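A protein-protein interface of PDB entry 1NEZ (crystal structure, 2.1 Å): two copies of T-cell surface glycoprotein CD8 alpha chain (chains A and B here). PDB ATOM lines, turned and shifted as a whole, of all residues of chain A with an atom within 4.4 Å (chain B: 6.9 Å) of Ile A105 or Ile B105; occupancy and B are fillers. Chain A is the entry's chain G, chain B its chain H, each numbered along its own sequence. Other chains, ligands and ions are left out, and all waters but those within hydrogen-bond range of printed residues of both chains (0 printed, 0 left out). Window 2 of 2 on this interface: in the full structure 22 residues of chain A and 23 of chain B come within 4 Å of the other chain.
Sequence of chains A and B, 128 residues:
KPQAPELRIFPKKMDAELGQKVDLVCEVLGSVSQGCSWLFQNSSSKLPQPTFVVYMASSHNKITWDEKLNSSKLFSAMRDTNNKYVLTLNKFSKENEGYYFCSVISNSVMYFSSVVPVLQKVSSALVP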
ATOM      1  N   GLN A  34     -20.573  16.679 -11.495  1.00  0.00           N
ATOM      2  CA  GLN A  34     -20.011  17.427 -12.598  1.00  0.00           C
ATOM      3  C   GLN A  34     -20.831  17.382 -13.861  1.00  0.00           C
ATOM      4  O   GLN A  34     -21.787  16.609 -13.971  1.00  0.00           O
ATOM      5  CB  GLN A  34     -18.551  17.017 -12.819  1.00  0.00           C
ATOM      6  CG  GLN A  34     -17.718  17.376 -11.581  1.00  0.00           C
ATOM      7  CD  GLN A  34     -16.258  17.056 -11.690  1.00  0.00           C
ATOM      8  OE1 GLN A  34     -15.462  17.816 -12.256  1.00  0.00           O
ATOM      9  NE2 GLN A  34     -15.881  15.930 -11.131  1.00  0.00           N
ATOM     10  N   VAL A 104     -18.701  11.897 -18.594  1.00  0.00           N
ATOM     11  CA  VAL A 104     -18.888  12.556 -17.310  1.00  0.00           C
ATOM     12  C   VAL A 104     -17.853  11.964 -16.380  1.00  0.00           C
ATOM     13  O   VAL A 104     -17.461  10.784 -16.505  1.00  0.00           O
ATOM     14  CB  VAL A 104     -20.287  12.351 -16.662  1.00  0.00           C
ATOM     15  CG1 VAL A 104     -21.397  12.806 -17.613  1.00  0.00           C
ATOM     16  CG2 VAL A 104     -20.466  10.932 -16.233  1.00  0.00           C
ATOM     17  N   ILE A 105     -17.366  12.802 -15.472  1.00  0.00           N
ATOM     18  CA  ILE A 105     -16.428  12.330 -14.504  1.00  0.00           C
ATOM     19  C   ILE A 105     -17.144  12.404 -13.192  1.00  0.00           C
ATOM     20  O   ILE A 105     -17.741  13.423 -12.850  1.00  0.00           O
ATOM     21  CB  ILE A 105     -15.172  13.172 -14.484  1.00  0.00           C
ATOM     22  CG1 ILE A 105     -14.384  12.893 -15.759  1.00  0.00           C
ATOM     23  CG2 ILE A 105     -14.348  12.847 -13.260  1.00  0.00           C
ATOM     24  CD1 ILE A 105     -13.194  13.756 -15.928  1.00  0.00           C
ATOM     25  N   SER A 106     -17.108  11.291 -12.471  1.00  0.00           N
ATOM     26  CA  SER A 106     -17.736  11.206 -11.157  1.00  0.00           C
ATOM     27  C   SER A 106     -16.783  10.440 -10.240  1.00  0.00           C
ATOM     28  O   SER A 106     -16.405   9.292 -10.530  1.00  0.00           O
ATOM     29  CB  SER A 106     -19.081  10.492 -11.253  1.00  0.00           C
ATOM     30  OG  SER A 106     -19.676  10.409  -9.976  1.00  0.00           O
ATOM     31  N   ASN A 107     -16.388  11.095  -9.147  1.00  0.00           N
ATOM     32  CA  ASN A 107     -15.447  10.529  -8.173  1.00  0.00           C
ATOM     33  C   ASN A 107     -14.196  10.001  -8.875  1.00  0.00           C
ATOM     34  O   ASN A 107     -13.800   8.845  -8.723  1.00  0.00           O
ATOM     35  CB  ASN A 107     -16.137   9.434  -7.362  1.00  0.00           C
ATOM     36  CG  ASN A 107     -17.211   9.991  -6.449  1.00  0.00           C
ATOM     37  OD1 ASN A 107     -18.386   9.625  -6.556  1.00  0.00           O
ATOM     38  ND2 ASN A 107     -16.818  10.888  -5.543  1.00  0.00           N
ATOM     39  N   SER A 108     -13.613  10.858  -9.703  1.00  0.00           N
ATOM     40  CA  SER A 108     -12.388  10.546 -10.416  1.00  0.00           C
ATOM     41  C   SER A 108     -12.390   9.449 -11.475  1.00  0.00           C
ATOM     42  O   SER A 108     -11.339   9.091 -12.023  1.00  0.00           O
ATOM     43  CB  SER A 108     -11.297  10.312  -9.379  1.00  0.00           C
ATOM     44  OG  SER A 108     -11.140  11.531  -8.666  1.00  0.00           O
ATOM     45  N   VAL A 109     -13.559   8.900 -11.766  1.00  0.00           N
ATOM     46  CA  VAL A 109     -13.641   7.900 -12.818  1.00  0.00           C
ATOM     47  C   VAL A 109     -14.319   8.578 -14.020  1.00  0.00           C
ATOM     48  O   VAL A 109     -15.351   9.248 -13.873  1.00  0.00           O
ATOM     49  CB  VAL A 109     -14.484   6.667 -12.382  1.00  0.00           C
ATOM     50  CG1 VAL A 109     -14.556   5.675 -13.506  1.00  0.00           C
ATOM     51  CG2 VAL A 109     -13.852   5.984 -11.138  1.00  0.00           C
ATOM     52  N   MET A 110     -13.709   8.449 -15.193  1.00  0.00           N
ATOM     53  CA  MET A 110     -14.281   8.981 -16.432  1.00  0.00           C
ATOM     54  C   MET A 110     -15.217   7.906 -16.990  1.00  0.00           C
ATOM     55  O   MET A 110     -14.804   6.774 -17.210  1.00  0.00           O
ATOM     56  CB  MET A 110     -13.213   9.243 -17.492  1.00  0.00           C
ATOM     57  CG  MET A 110     -12.303  10.427 -17.228  1.00  0.00           C
ATOM     58  SD  MET A 110     -11.181  10.662 -18.608  1.00  0.00           S
ATOM     59  CE  MET A 110     -12.358  11.185 -19.884  1.00  0.00           C
ATOM     60  N   PRO B   5      -2.305  22.575 -21.272  1.00  0.00           N
ATOM     61  CA  PRO B   5      -1.191  21.752 -20.809  1.00  0.00           C
ATOM     62  C   PRO B   5      -0.705  20.974 -22.033  1.00  0.00           C
ATOM     63  O   PRO B   5      -1.427  20.864 -23.044  1.00  0.00           O
ATOM     64  CB  PRO B   5      -1.850  20.834 -19.798  1.00  0.00           C
ATOM     65  CG  PRO B   5      -3.203  20.635 -20.376  1.00  0.00           C
ATOM     66  CD  PRO B   5      -3.590  22.042 -20.793  1.00  0.00           C
ATOM     67  N   VAL B  32      -1.133  23.765 -15.305  1.00  0.00           N
ATOM     68  CA  VAL B  32      -2.539  24.141 -15.379  1.00  0.00           C
ATOM     69  C   VAL B  32      -3.462  22.946 -15.359  1.00  0.00           C
ATOM     70  O   VAL B  32      -4.649  23.067 -15.627  1.00  0.00           O
ATOM     71  CB  VAL B  32      -2.809  24.992 -16.624  1.00  0.00           C
ATOM     72  CG1 VAL B  32      -2.027  26.317 -16.483  1.00  0.00           C
ATOM     73  CG2 VAL B  32      -2.346  24.233 -17.895  1.00  0.00           C
ATOM     74  N   SER B  33      -2.911  21.776 -15.071  1.00  0.00           N
ATOM     75  CA  SER B  33      -3.752  20.589 -14.961  1.00  0.00           C
ATOM     76  C   SER B  33      -3.290  19.834 -13.721  1.00  0.00           C
ATOM     77  O   SER B  33      -2.137  19.975 -13.299  1.00  0.00           O
ATOM     78  CB  SER B  33      -3.622  19.690 -16.204  1.00  0.00           C
ATOM     79  OG  SER B  33      -2.279  19.303 -16.459  1.00  0.00           O
ATOM     80  N   GLN B  34      -4.183  19.060 -13.120  1.00  0.00           N
ATOM     81  CA  GLN B  34      -3.789  18.270 -11.958  1.00  0.00           C
ATOM     82  C   GLN B  34      -4.251  16.848 -12.136  1.00  0.00           C
ATOM     83  O   GLN B  34      -5.422  16.613 -12.448  1.00  0.00           O
ATOM     84  CB  GLN B  34      -4.358  18.855 -10.670  1.00  0.00           C
ATOM     85  CG  GLN B  34      -3.546  20.049 -10.222  1.00  0.00           C
ATOM     86  CD  GLN B  34      -4.191  20.857  -9.081  1.00  0.00           C
ATOM     87  OE1 GLN B  34      -3.521  21.668  -8.437  1.00  0.00           O
ATOM     88  NE2 GLN B  34      -5.483  20.658  -8.856  1.00  0.00           N
ATOM     89  N   GLY B  35      -3.317  15.904 -11.970  1.00  0.00           N
ATOM     90  CA  GLY B  35      -3.650  14.493 -12.109  1.00  0.00           C
ATOM     91  C   GLY B  35      -3.566  14.058 -13.559  1.00  0.00           C
ATOM     92  O   GLY B  35      -3.345  14.900 -14.418  1.00  0.00           O
ATOM     93  N   CYS B  36      -3.768  12.766 -13.831  1.00  0.00           N
ATOM     94  CA  CYS B  36      -3.676  12.217 -15.184  1.00  0.00           C
ATOM     95  C   CYS B  36      -4.485  10.928 -15.323  1.00  0.00           C
ATOM     96  O   CYS B  36      -4.457  10.071 -14.432  1.00  0.00           O
ATOM     97  CB  CYS B  36      -2.192  11.951 -15.508  1.00  0.00           C
ATOM     98  SG  CYS B  36      -1.803  11.101 -17.079  1.00  0.00           S
ATOM     99  N   SER B  37      -5.224  10.787 -16.426  1.00  0.00           N
ATOM    100  CA  SER B  37      -6.015   9.576 -16.650  1.00  0.00           C
ATOM    101  C   SER B  37      -5.492   8.795 -17.832  1.00  0.00           C
ATOM    102  O   SER B  37      -5.124   9.369 -18.837  1.00  0.00           O
ATOM    103  CB  SER B  37      -7.493   9.904 -16.904  1.00  0.00           C
ATOM    104  OG  SER B  37      -8.083  10.553 -15.800  1.00  0.00           O
ATOM    105  N   SER B 103      -4.819  11.442 -20.734  1.00  0.00           N
ATOM    106  CA  SER B 103      -5.646  12.613 -20.825  1.00  0.00           C
ATOM    107  C   SER B 103      -5.614  13.381 -19.505  1.00  0.00           C
ATOM    108  O   SER B 103      -5.572  12.779 -18.416  1.00  0.00           O
ATOM    109  CB  SER B 103      -7.092  12.204 -21.136  1.00  0.00           C
ATOM    110  OG  SER B 103      -7.986  13.296 -20.993  1.00  0.00           O
ATOM    111  N   VAL B 104      -5.603  14.709 -19.603  1.00  0.00           N
ATOM    112  CA  VAL B 104      -5.670  15.527 -18.398  1.00  0.00           C
ATOM    113  C   VAL B 104      -6.748  16.574 -18.675  1.00  0.00           C
ATOM    114  O   VAL B 104      -7.104  16.833 -19.825  1.00  0.00           O
ATOM    115  CB  VAL B 104      -4.304  16.237 -18.050  1.00  0.00           C
ATOM    116  CG1 VAL B 104      -3.157  15.220 -18.046  1.00  0.00           C
ATOM    117  CG2 VAL B 104      -4.019  17.382 -19.017  1.00  0.00           C
ATOM    118  N   ILE B 105      -7.296  17.144 -17.614  1.00  0.00           N
ATOM    119  CA  ILE B 105      -8.295  18.178 -17.760  1.00  0.00           C
ATOM    120  C   ILE B 105      -7.653  19.490 -17.317  1.00  0.00           C
ATOM    121  O   ILE B 105      -6.834  19.511 -16.399  1.00  0.00           O
ATOM    122  CB  ILE B 105      -9.524  17.864 -16.891  1.00  0.00           C
ATOM    123  CG1 ILE B 105     -10.328  16.726 -17.541  1.00  0.00           C
ATOM    124  CG2 ILE B 105     -10.370  19.104 -16.711  1.00  0.00           C
ATOM    125  CD1 ILE B 105     -11.468  16.324 -16.719  1.00  0.00           C
ATOM    126  N   SER B 106      -7.978  20.577 -18.005  1.00  0.00           N
ATOM    127  CA  SER B 106      -7.462  21.880 -17.618  1.00  0.00           C
ATOM    128  C   SER B 106      -8.558  22.900 -17.882  1.00  0.00           C
ATOM    129  O   SER B 106      -8.987  23.085 -19.016  1.00  0.00           O
ATOM    130  CB  SER B 106      -6.205  22.246 -18.405  1.00  0.00           C
ATOM    131  OG  SER B 106      -5.899  23.604 -18.180  1.00  0.00           O
ATOM    132  N   ASN B 107      -9.016  23.536 -16.809  1.00  0.00           N
ATOM    133  CA  ASN B 107     -10.072  24.521 -16.886  1.00  0.00           C
ATOM    134  C   ASN B 107     -11.286  24.058 -17.702  1.00  0.00           C
ATOM    135  O   ASN B 107     -11.788  24.759 -18.592  1.00  0.00           O
ATOM    136  CB  ASN B 107      -9.471  25.843 -17.383  1.00  0.00           C
ATOM    137  CG  ASN B 107      -8.305  26.295 -16.492  1.00  0.00           C
ATOM    138  OD1 ASN B 107      -8.225  25.881 -15.329  1.00  0.00           O
ATOM    139  ND2 ASN B 107      -7.402  27.129 -17.021  1.00  0.00           N
ATOM    140  N   SER B 108     -11.737  22.846 -17.364  1.00  0.00           N
ATOM    141  CA  SER B 108     -12.921  22.214 -17.948  1.00  0.00           C
ATOM    142  C   SER B 108     -12.760  21.600 -19.308  1.00  0.00           C
ATOM    143  O   SER B 108     -13.694  20.977 -19.809  1.00  0.00           O
ATOM    144  CB  SER B 108     -14.072  23.220 -17.989  1.00  0.00           C
ATOM    145  OG  SER B 108     -14.400  23.627 -16.681  1.00  0.00           O
ATOM    146  N   VAL B 109     -11.601  21.798 -19.931  1.00  0.00           N
ATOM    147  CA  VAL B 109     -11.334  21.215 -21.237  1.00  0.00           C
ATOM    148  C   VAL B 109     -10.512  19.940 -21.103  1.00  0.00           C
ATOM    149  O   VAL B 109      -9.532  19.897 -20.327  1.00  0.00           O
ATOM    150  CB  VAL B 109     -10.573  22.209 -22.165  1.00  0.00           C
ATOM    151  CG1 VAL B 109     -10.195  21.552 -23.459  1.00  0.00           C
ATOM    152  CG2 VAL B 109     -11.434  23.460 -22.443  1.00  0.00           C
ATOM    153  N   MET B 110     -10.903  18.899 -21.851  1.00  0.00           N
ATOM    154  CA  MET B 110     -10.169  17.632 -21.834  1.00  0.00           C
ATOM    155  C   MET B 110      -9.119  17.688 -22.917  1.00  0.00           C
ATOM    156  O   MET B 110      -9.402  18.088 -24.046  1.00  0.00           O
ATOM    157  CB  MET B 110     -11.084  16.403 -22.102  1.00  0.00           C
ATOM    158  CG  MET B 110     -12.198  16.166 -21.069  1.00  0.00           C
ATOM    159  SD  MET B 110     -13.040  14.583 -21.314  1.00  0.00           S
ATOM    160  CE  MET B 110     -13.863  14.328 -19.728  1.00  0.00           C
ATOM    161  N   TYR B 111      -7.903  17.284 -22.555  1.00  0.00           N
ATOM    162  CA  TYR B 111      -6.753  17.256 -23.439  1.00  0.00           C
ATOM    163  C   TYR B 111      -6.309  15.790 -23.538  1.00  0.00           C
ATOM    164  O   TYR B 111      -6.439  15.013 -22.566  1.00  0.00           O
ATOM    165  CB  TYR B 111      -5.629  18.114 -22.846  1.00  0.00           C
ATOM    166  CG  TYR B 111      -5.936  19.597 -22.898  1.00  0.00           C
ATOM    167  CD1 TYR B 111      -5.552  20.370 -24.005  1.00  0.00           C
ATOM    168  CD2 TYR B 111      -6.668  20.211 -21.894  1.00  0.00           C
ATOM    169  CE1 TYR B 111      -5.897  21.710 -24.096  1.00  0.00           C
ATOM    170  CE2 TYR B 111      -7.020  21.567 -21.977  1.00  0.00           C
ATOM    171  CZ  TYR B 111      -6.631  22.299 -23.078  1.00  0.00           C
ATOM    172  OH  TYR B 111      -6.996  23.617 -23.177  1.00  0.00           O
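Ile B105 touches Ile A105 (CD1 to CD1, 3.2 Å). Met B110 touches Ile A105. Met B110 touches Met A110 (CE to CE, 3.5 Å).
Ser A108 touches none of the printed residues of chain B. Of the printed residues of chain B, Met A110 touches Met B110. Of the printed residues of chain A, Ile B105 touches Ile A105. Of the printed residues of chain A, Met B110 touches Ile A105 (3.9 Å) and Met A110 (3.5 Å). The nearest printed residue of chain A that does not touch Met B110 is Val A104 (5.5 Å).
Of the 8 printed residues of chain A, 2 touch a printed residue of chain B. Printed residues of chain A that touch a printed residue of chain B: Ile A105 and Met A110. Hydrophobic or aromatic side chains of chain A within 4 Å of the printed part of chain B: Ile A105 and Met A110. Among the printed residues, no Asp or Glu carboxylate lies within 4 Å of a Lys or Arg side-chain nitrogen of the other chain.
Ile B105 touches its own counterpart, Ile A105. Ile A105 touches Met B110, but with the chains exchanged Met A110 does not touch Ile B105 (6.0 Å). Met B110 touches its own counterpart, Met A110. Positions printed for both chains: 34, 104, 105, 106, 107, 108, 109 and 110.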
